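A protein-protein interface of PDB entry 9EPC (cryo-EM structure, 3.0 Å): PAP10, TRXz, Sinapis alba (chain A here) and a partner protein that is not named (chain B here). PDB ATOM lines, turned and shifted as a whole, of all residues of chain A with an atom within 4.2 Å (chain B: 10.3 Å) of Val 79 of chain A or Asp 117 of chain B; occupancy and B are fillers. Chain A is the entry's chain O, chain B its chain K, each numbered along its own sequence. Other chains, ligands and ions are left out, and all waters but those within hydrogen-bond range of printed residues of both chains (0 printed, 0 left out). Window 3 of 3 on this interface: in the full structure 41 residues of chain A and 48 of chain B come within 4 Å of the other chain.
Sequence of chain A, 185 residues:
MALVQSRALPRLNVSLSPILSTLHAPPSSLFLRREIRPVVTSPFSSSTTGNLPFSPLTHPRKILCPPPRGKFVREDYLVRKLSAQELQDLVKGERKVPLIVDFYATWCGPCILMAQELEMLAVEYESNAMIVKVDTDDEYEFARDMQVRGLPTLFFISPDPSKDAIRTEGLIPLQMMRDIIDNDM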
ATOM      1  N   TYR A  77       9.609  19.411  15.508  1.00  0.00           N
ATOM      2  CA  TYR A  77      10.110  18.599  16.606  1.00  0.00           C
ATOM      3  C   TYR A  77      11.230  17.701  16.112  1.00  0.00           C
ATOM      4  O   TYR A  77      11.100  17.060  15.064  1.00  0.00           O
ATOM      5  CB  TYR A  77       8.982  17.766  17.216  1.00  0.00           C
ATOM      6  CG  TYR A  77       7.811  18.609  17.654  1.00  0.00           C
ATOM      7  CD1 TYR A  77       7.777  19.176  18.917  1.00  0.00           C
ATOM      8  CD2 TYR A  77       6.748  18.851  16.798  1.00  0.00           C
ATOM      9  CE1 TYR A  77       6.716  19.952  19.321  1.00  0.00           C
ATOM     10  CE2 TYR A  77       5.681  19.627  17.194  1.00  0.00           C
ATOM     11  CZ  TYR A  77       5.671  20.175  18.456  1.00  0.00           C
ATOM     12  OH  TYR A  77       4.610  20.950  18.858  1.00  0.00           O
ATOM     13  N   LEU A  78      12.325  17.657  16.868  1.00  0.00           N
ATOM     14  CA  LEU A  78      13.475  16.842  16.510  1.00  0.00           C
ATOM     15  C   LEU A  78      13.547  15.530  17.275  1.00  0.00           C
ATOM     16  O   LEU A  78      14.182  14.587  16.792  1.00  0.00           O
ATOM     17  CB  LEU A  78      14.770  17.626  16.746  1.00  0.00           C
ATOM     18  CG  LEU A  78      14.872  18.972  16.032  1.00  0.00           C
ATOM     19  CD1 LEU A  78      16.236  19.589  16.262  1.00  0.00           C
ATOM     20  CD2 LEU A  78      14.596  18.810  14.550  1.00  0.00           C
ATOM     21  N   VAL A  79      12.921  15.445  18.445  1.00  0.00           N
ATOM     22  CA  VAL A  79      12.949  14.226  19.246  1.00  0.00           C
ATOM     23  C   VAL A  79      11.973  13.234  18.625  1.00  0.00           C
ATOM     24  O   VAL A  79      10.758  13.449  18.640  1.00  0.00           O
ATOM     25  CB  VAL A  79      12.602  14.507  20.711  1.00  0.00           C
ATOM     26  CG1 VAL A  79      12.617  13.221  21.509  1.00  0.00           C
ATOM     27  CG2 VAL A  79      13.579  15.508  21.297  1.00  0.00           C
ATOM     28  N   ARG A  80      12.501  12.143  18.083  1.00  0.00           N
ATOM     29  CA  ARG A  80      11.702  11.163  17.363  1.00  0.00           C
ATOM     30  C   ARG A  80      11.147  10.121  18.325  1.00  0.00           C
ATOM     31  O   ARG A  80      11.878   9.599  19.173  1.00  0.00           O
ATOM     32  CB  ARG A  80      12.544  10.488  16.281  1.00  0.00           C
ATOM     33  CG  ARG A  80      11.839   9.362  15.549  1.00  0.00           C
ATOM     34  CD  ARG A  80      12.743   8.721  14.506  1.00  0.00           C
ATOM     35  NE  ARG A  80      13.896   8.055  15.101  1.00  0.00           N
ATOM     36  CZ  ARG A  80      15.107   8.587  15.193  1.00  0.00           C
ATOM     37  NH1 ARG A  80      15.364   9.803  14.738  1.00  0.00           N
ATOM     38  NH2 ARG A  80      16.085   7.883  15.755  1.00  0.00           N
ATOM     39  N   LYS A  81       9.858   9.827  18.192  1.00  0.00           N
ATOM     40  CA  LYS A  81       9.223   8.801  19.007  1.00  0.00           C
ATOM     41  C   LYS A  81       9.472   7.428  18.399  1.00  0.00           C
ATOM     42  O   LYS A  81       9.309   7.236  17.191  1.00  0.00           O
ATOM     43  CB  LYS A  81       7.724   9.066  19.121  1.00  0.00           C
ATOM     44  CG  LYS A  81       6.957   7.978  19.843  1.00  0.00           C
ATOM     45  CD  LYS A  81       5.470   8.270  19.846  1.00  0.00           C
ATOM     46  CE  LYS A  81       4.694   7.179  20.555  1.00  0.00           C
ATOM     47  NZ  LYS A  81       3.236   7.460  20.566  1.00  0.00           N
ATOM     48  N   LEU A 118      14.093  18.434  26.032  1.00  0.00           N
ATOM     49  CA  LEU A 118      14.710  17.529  25.067  1.00  0.00           C
ATOM     50  C   LEU A 118      14.788  18.167  23.689  1.00  0.00           C
ATOM     51  O   LEU A 118      15.795  18.020  22.988  1.00  0.00           O
ATOM     52  CB  LEU A 118      13.946  16.209  25.005  1.00  0.00           C
ATOM     53  CG  LEU A 118      14.245  15.204  26.117  1.00  0.00           C
ATOM     54  CD1 LEU A 118      15.719  15.209  26.473  1.00  0.00           C
ATOM     55  CD2 LEU A 118      13.416  15.496  27.329  1.00  0.00           C
ATOM     56  N   GLU A 119      13.737  18.878  23.281  1.00  0.00           N
ATOM     57  CA  GLU A 119      13.793  19.611  22.023  1.00  0.00           C
ATOM     58  C   GLU A 119      14.913  20.639  22.051  1.00  0.00           C
ATOM     59  O   GLU A 119      15.672  20.770  21.084  1.00  0.00           O
ATOM     60  CB  GLU A 119      12.454  20.292  21.749  1.00  0.00           C
ATOM     61  CG  GLU A 119      11.248  19.378  21.845  1.00  0.00           C
ATOM     62  CD  GLU A 119      11.022  18.570  20.587  1.00  0.00           C
ATOM     63  OE1 GLU A 119      11.635  18.898  19.552  1.00  0.00           O
ATOM     64  OE2 GLU A 119      10.227  17.609  20.634  1.00  0.00           O
ATOM     65  N   ILE A 131      18.599  11.764  20.428  1.00  0.00           N
ATOM     66  CA  ILE A 131      17.568  11.819  21.457  1.00  0.00           C
ATOM     67  C   ILE A 131      16.294  11.226  20.880  1.00  0.00           C
ATOM     68  O   ILE A 131      15.810  11.671  19.832  1.00  0.00           O
ATOM     69  CB  ILE A 131      17.332  13.255  21.948  1.00  0.00           C
ATOM     70  CG1 ILE A 131      18.623  13.840  22.517  1.00  0.00           C
ATOM     71  CG2 ILE A 131      16.236  13.283  22.993  1.00  0.00           C
ATOM     72  CD1 ILE A 131      18.456  15.223  23.086  1.00  0.00           C
ATOM     73  N   VAL A 132      15.753  10.217  21.561  1.00  0.00           N
ATOM     74  CA  VAL A 132      14.497   9.591  21.182  1.00  0.00           C
ATOM     75  C   VAL A 132      13.620   9.506  22.422  1.00  0.00           C
ATOM     76  O   VAL A 132      14.095   9.594  23.554  1.00  0.00           O
ATOM     77  CB  VAL A 132      14.699   8.192  20.564  1.00  0.00           C
ATOM     78  CG1 VAL A 132      15.564   8.286  19.324  1.00  0.00           C
ATOM     79  CG2 VAL A 132      15.320   7.255  21.576  1.00  0.00           C
ATOM     80  N   LYS A 133      12.322   9.340  22.194  1.00  0.00           N
ATOM     81  CA  LYS A 133      11.361   9.247  23.281  1.00  0.00           C
ATOM     82  C   LYS A 133      10.445   8.054  23.061  1.00  0.00           C
ATOM     83  O   LYS A 133      10.137   7.685  21.926  1.00  0.00           O
ATOM     84  CB  LYS A 133      10.533  10.528  23.415  1.00  0.00           C
ATOM     85  CG  LYS A 133       9.781  10.918  22.163  1.00  0.00           C
ATOM     86  CD  LYS A 133       9.087  12.253  22.344  1.00  0.00           C
ATOM     87  CE  LYS A 133       8.415  12.698  21.062  1.00  0.00           C
ATOM     88  NZ  LYS A 133       7.819  14.054  21.190  1.00  0.00           N
ATOM     89  N   PRO B 113      -4.477   8.753  23.987  1.00  0.00           N
ATOM     90  CA  PRO B 113      -3.312   9.637  24.070  1.00  0.00           C
ATOM     91  C   PRO B 113      -3.454  10.815  23.123  1.00  0.00           C
ATOM     92  O   PRO B 113      -4.097  10.727  22.073  1.00  0.00           O
ATOM     93  CB  PRO B 113      -2.144   8.731  23.657  1.00  0.00           C
ATOM     94  CG  PRO B 113      -2.685   7.334  23.698  1.00  0.00           C
ATOM     95  CD  PRO B 113      -4.132   7.461  23.376  1.00  0.00           C
ATOM     96  N   MET B 114      -2.841  11.929  23.504  1.00  0.00           N
ATOM     97  CA  MET B 114      -2.829  13.115  22.660  1.00  0.00           C
ATOM     98  C   MET B 114      -1.703  12.989  21.636  1.00  0.00           C
ATOM     99  O   MET B 114      -1.110  11.922  21.458  1.00  0.00           O
ATOM    100  CB  MET B 114      -2.710  14.372  23.515  1.00  0.00           C
ATOM    101  CG  MET B 114      -3.899  14.593  24.425  1.00  0.00           C
ATOM    102  SD  MET B 114      -5.452  14.492  23.518  1.00  0.00           S
ATOM    103  CE  MET B 114      -6.636  14.568  24.856  1.00  0.00           C
ATOM    104  N   HIS B 115      -1.402  14.080  20.942  1.00  0.00           N
ATOM    105  CA  HIS B 115      -0.397  14.031  19.894  1.00  0.00           C
ATOM    106  C   HIS B 115       0.968  13.709  20.496  1.00  0.00           C
ATOM    107  O   HIS B 115       1.331  14.256  21.544  1.00  0.00           O
ATOM    108  CB  HIS B 115      -0.340  15.357  19.139  1.00  0.00           C
ATOM    109  CG  HIS B 115       0.429  15.288  17.857  1.00  0.00           C
ATOM    110  ND1 HIS B 115       1.801  15.378  17.807  1.00  0.00           N
ATOM    111  CD2 HIS B 115       0.015  15.132  16.578  1.00  0.00           C
ATOM    112  CE1 HIS B 115       2.202  15.282  16.553  1.00  0.00           C
ATOM    113  NE2 HIS B 115       1.137  15.134  15.787  1.00  0.00           N
ATOM    114  N   PRO B 116       1.740  12.814  19.875  1.00  0.00           N
ATOM    115  CA  PRO B 116       3.039  12.440  20.459  1.00  0.00           C
ATOM    116  C   PRO B 116       4.005  13.601  20.600  1.00  0.00           C
ATOM    117  O   PRO B 116       4.776  13.645  21.565  1.00  0.00           O
ATOM    118  CB  PRO B 116       3.568  11.386  19.477  1.00  0.00           C
ATOM    119  CG  PRO B 116       2.362  10.883  18.765  1.00  0.00           C
ATOM    120  CD  PRO B 116       1.442  12.051  18.653  1.00  0.00           C
ATOM    121  N   ASP B 117       3.988  14.545  19.663  1.00  0.00           N
ATOM    122  CA  ASP B 117       4.950  15.638  19.641  1.00  0.00           C
ATOM    123  C   ASP B 117       4.380  16.952  20.148  1.00  0.00           C
ATOM    124  O   ASP B 117       5.074  17.694  20.848  1.00  0.00           O
ATOM    125  CB  ASP B 117       5.484  15.840  18.221  1.00  0.00           C
ATOM    126  CG  ASP B 117       6.211  14.623  17.696  1.00  0.00           C
ATOM    127  OD1 ASP B 117       6.888  13.945  18.494  1.00  0.00           O
ATOM    128  OD2 ASP B 117       6.104  14.342  16.485  1.00  0.00           O
ATOM    129  N   ILE B 118       3.128  17.258  19.820  1.00  0.00           N
ATOM    130  CA  ILE B 118       2.545  18.549  20.157  1.00  0.00           C
ATOM    131  C   ILE B 118       2.115  18.538  21.616  1.00  0.00           C
ATOM    132  O   ILE B 118       0.994  18.138  21.943  1.00  0.00           O
ATOM    133  CB  ILE B 118       1.362  18.879  19.232  1.00  0.00           C
ATOM    134  CG1 ILE B 118       1.795  18.786  17.770  1.00  0.00           C
ATOM    135  CG2 ILE B 118       0.829  20.262  19.527  1.00  0.00           C
ATOM    136  CD1 ILE B 118       0.696  19.102  16.792  1.00  0.00           C
ATOM    137  N   TYR B 119       3.006  18.981  22.503  1.00  0.00           N
ATOM    138  CA  TYR B 119       2.709  18.965  23.928  1.00  0.00           C
ATOM    139  C   TYR B 119       1.702  20.029  24.336  1.00  0.00           C
ATOM    140  O   TYR B 119       1.214  19.988  25.469  1.00  0.00           O
ATOM    141  CB  TYR B 119       3.995  19.128  24.738  1.00  0.00           C
ATOM    142  CG  TYR B 119       4.918  20.205  24.230  1.00  0.00           C
ATOM    143  CD1 TYR B 119       4.700  21.536  24.544  1.00  0.00           C
ATOM    144  CD2 TYR B 119       6.015  19.888  23.445  1.00  0.00           C
ATOM    145  CE1 TYR B 119       5.543  22.520  24.083  1.00  0.00           C
ATOM    146  CE2 TYR B 119       6.863  20.867  22.983  1.00  0.00           C
ATOM    147  CZ  TYR B 119       6.622  22.180  23.304  1.00  0.00           C
ATOM    148  OH  TYR B 119       7.467  23.160  22.844  1.00  0.00           O
ATOM    149  N   SER B 120       1.381  20.978  23.456  1.00  0.00           N
ATOM    150  CA  SER B 120       0.359  21.962  23.785  1.00  0.00           C
ATOM    151  C   SER B 120      -1.020  21.332  23.910  1.00  0.00           C
ATOM    152  O   SER B 120      -1.887  21.896  24.584  1.00  0.00           O
ATOM    153  CB  SER B 120       0.332  23.071  22.734  1.00  0.00           C
ATOM    154  OG  SER B 120      -0.157  22.591  21.497  1.00  0.00           O
ATOM    155  N   GLN B 121      -1.243  20.179  23.278  1.00  0.00           N
ATOM    156  CA  GLN B 121      -2.511  19.476  23.411  1.00  0.00           C
ATOM    157  C   GLN B 121      -2.608  18.685  24.705  1.00  0.00           C
ATOM    158  O   GLN B 121      -3.707  18.260  25.073  1.00  0.00           O
ATOM    159  CB  GLN B 121      -2.716  18.527  22.232  1.00  0.00           C
ATOM    160  CG  GLN B 121      -2.748  19.202  20.881  1.00  0.00           C
ATOM    161  CD  GLN B 121      -2.946  18.212  19.756  1.00  0.00           C
ATOM    162  OE1 GLN B 121      -3.102  17.014  19.989  1.00  0.00           O
ATOM    163  NE2 GLN B 121      -2.940  18.707  18.524  1.00  0.00           N
ATOM    164  N   TRP B 122      -1.491  18.479  25.401  1.00  0.00           N
ATOM    165  CA  TRP B 122      -1.490  17.627  26.581  1.00  0.00           C
ATOM    166  C   TRP B 122      -2.223  18.251  27.759  1.00  0.00           C
ATOM    167  O   TRP B 122      -2.500  17.545  28.732  1.00  0.00           O
ATOM    168  CB  TRP B 122      -0.054  17.286  26.976  1.00  0.00           C
ATOM    169  CG  TRP B 122       0.692  16.533  25.915  1.00  0.00           C
ATOM    170  CD1 TRP B 122       0.203  16.103  24.719  1.00  0.00           C
ATOM    171  CD2 TRP B 122       2.062  16.121  25.958  1.00  0.00           C
ATOM    172  NE1 TRP B 122       1.182  15.453  24.013  1.00  0.00           N
ATOM    173  CE2 TRP B 122       2.333  15.451  24.752  1.00  0.00           C
ATOM    174  CE3 TRP B 122       3.087  16.257  26.897  1.00  0.00           C
ATOM    175  CZ2 TRP B 122       3.582  14.915  24.463  1.00  0.00           C
ATOM    176  CZ3 TRP B 122       4.324  15.726  26.607  1.00  0.00           C
ATOM    177  CH2 TRP B 122       4.563  15.065  25.401  1.00  0.00           C
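The side-chain amino group of Lys 133 of chain A is in salt-bridge range of the side-chain carboxylate of Asp 117 of chain B.
O of Pro 116 of chain B sits at hydrogen-bond distance from NZ of Lys 133 of chain A (3.1 Å).
A ring nitrogen (ND1) of His 115 of chain B is in hydrogen-bond range of the backbone NH (N) of Asp 117 of chain B (3.0 Å).
The backbone carbonyl oxygen (O) of Ile 118 of chain B sits at hydrogen-bond distance from the indole nitrogen (NE1) of Trp 122 of chain B (3.4 Å).
O of Arg 80 of chain A lies within hydrogen-bond range of N of Lys 133 of chain A.
N of Ile 118 of chain B is in hydrogen-bond range of ND1 of His 115 of chain B.
Among the printed residues, merely in contact across the chains: Tyr 77 of chain A with Asp 117 of chain B (3.2 Å), Tyr 77 of chain A with Ile 118 of chain B (3.4 Å), Lys 81 of chain A with Pro 116 of chain B (3.7 Å), Tyr 77 of chain A with Tyr 119 of chain B (3.8 Å) and Val 79 of chain A with Asp 117 of chain B (3.9 Å).
Of chain B, only Asp 117, Ile 118 and Tyr 119 come within 4 Å of Tyr 77 of chain A.
No residue of chain B comes within 4 Å of Leu 78 of chain A.
Of chain B, only Asp 117 comes within 4 Å of Val 79 of chain A.
Arg 80 of chain A touches none of the printed residues of chain B.
No residue of chain B comes within 4 Å of Leu 118 of chain A.
Of the printed residues of chain A, Pro 116 of chain B touches Lys 81 (3.7 Å) and Lys 133 (3.1 Å).
Of chain A, only Tyr 77, Val 79 and Lys 133 come within 4 Å of Asp 117 of chain B.
Of the printed residues of chain A, Ile 118 of chain B touches Tyr 77.
Gln 121 of chain B touches none of the printed residues of chain A.
The nearest printed residue of chain B that does not touch Lys 81 of chain A is Asp 117 of chain B (5.0 Å).
Hydrophobic or aromatic side chains of chain A that line the printed part of chain B: Tyr 77.
Among the printed residues, 7 pairs touch across the chains.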
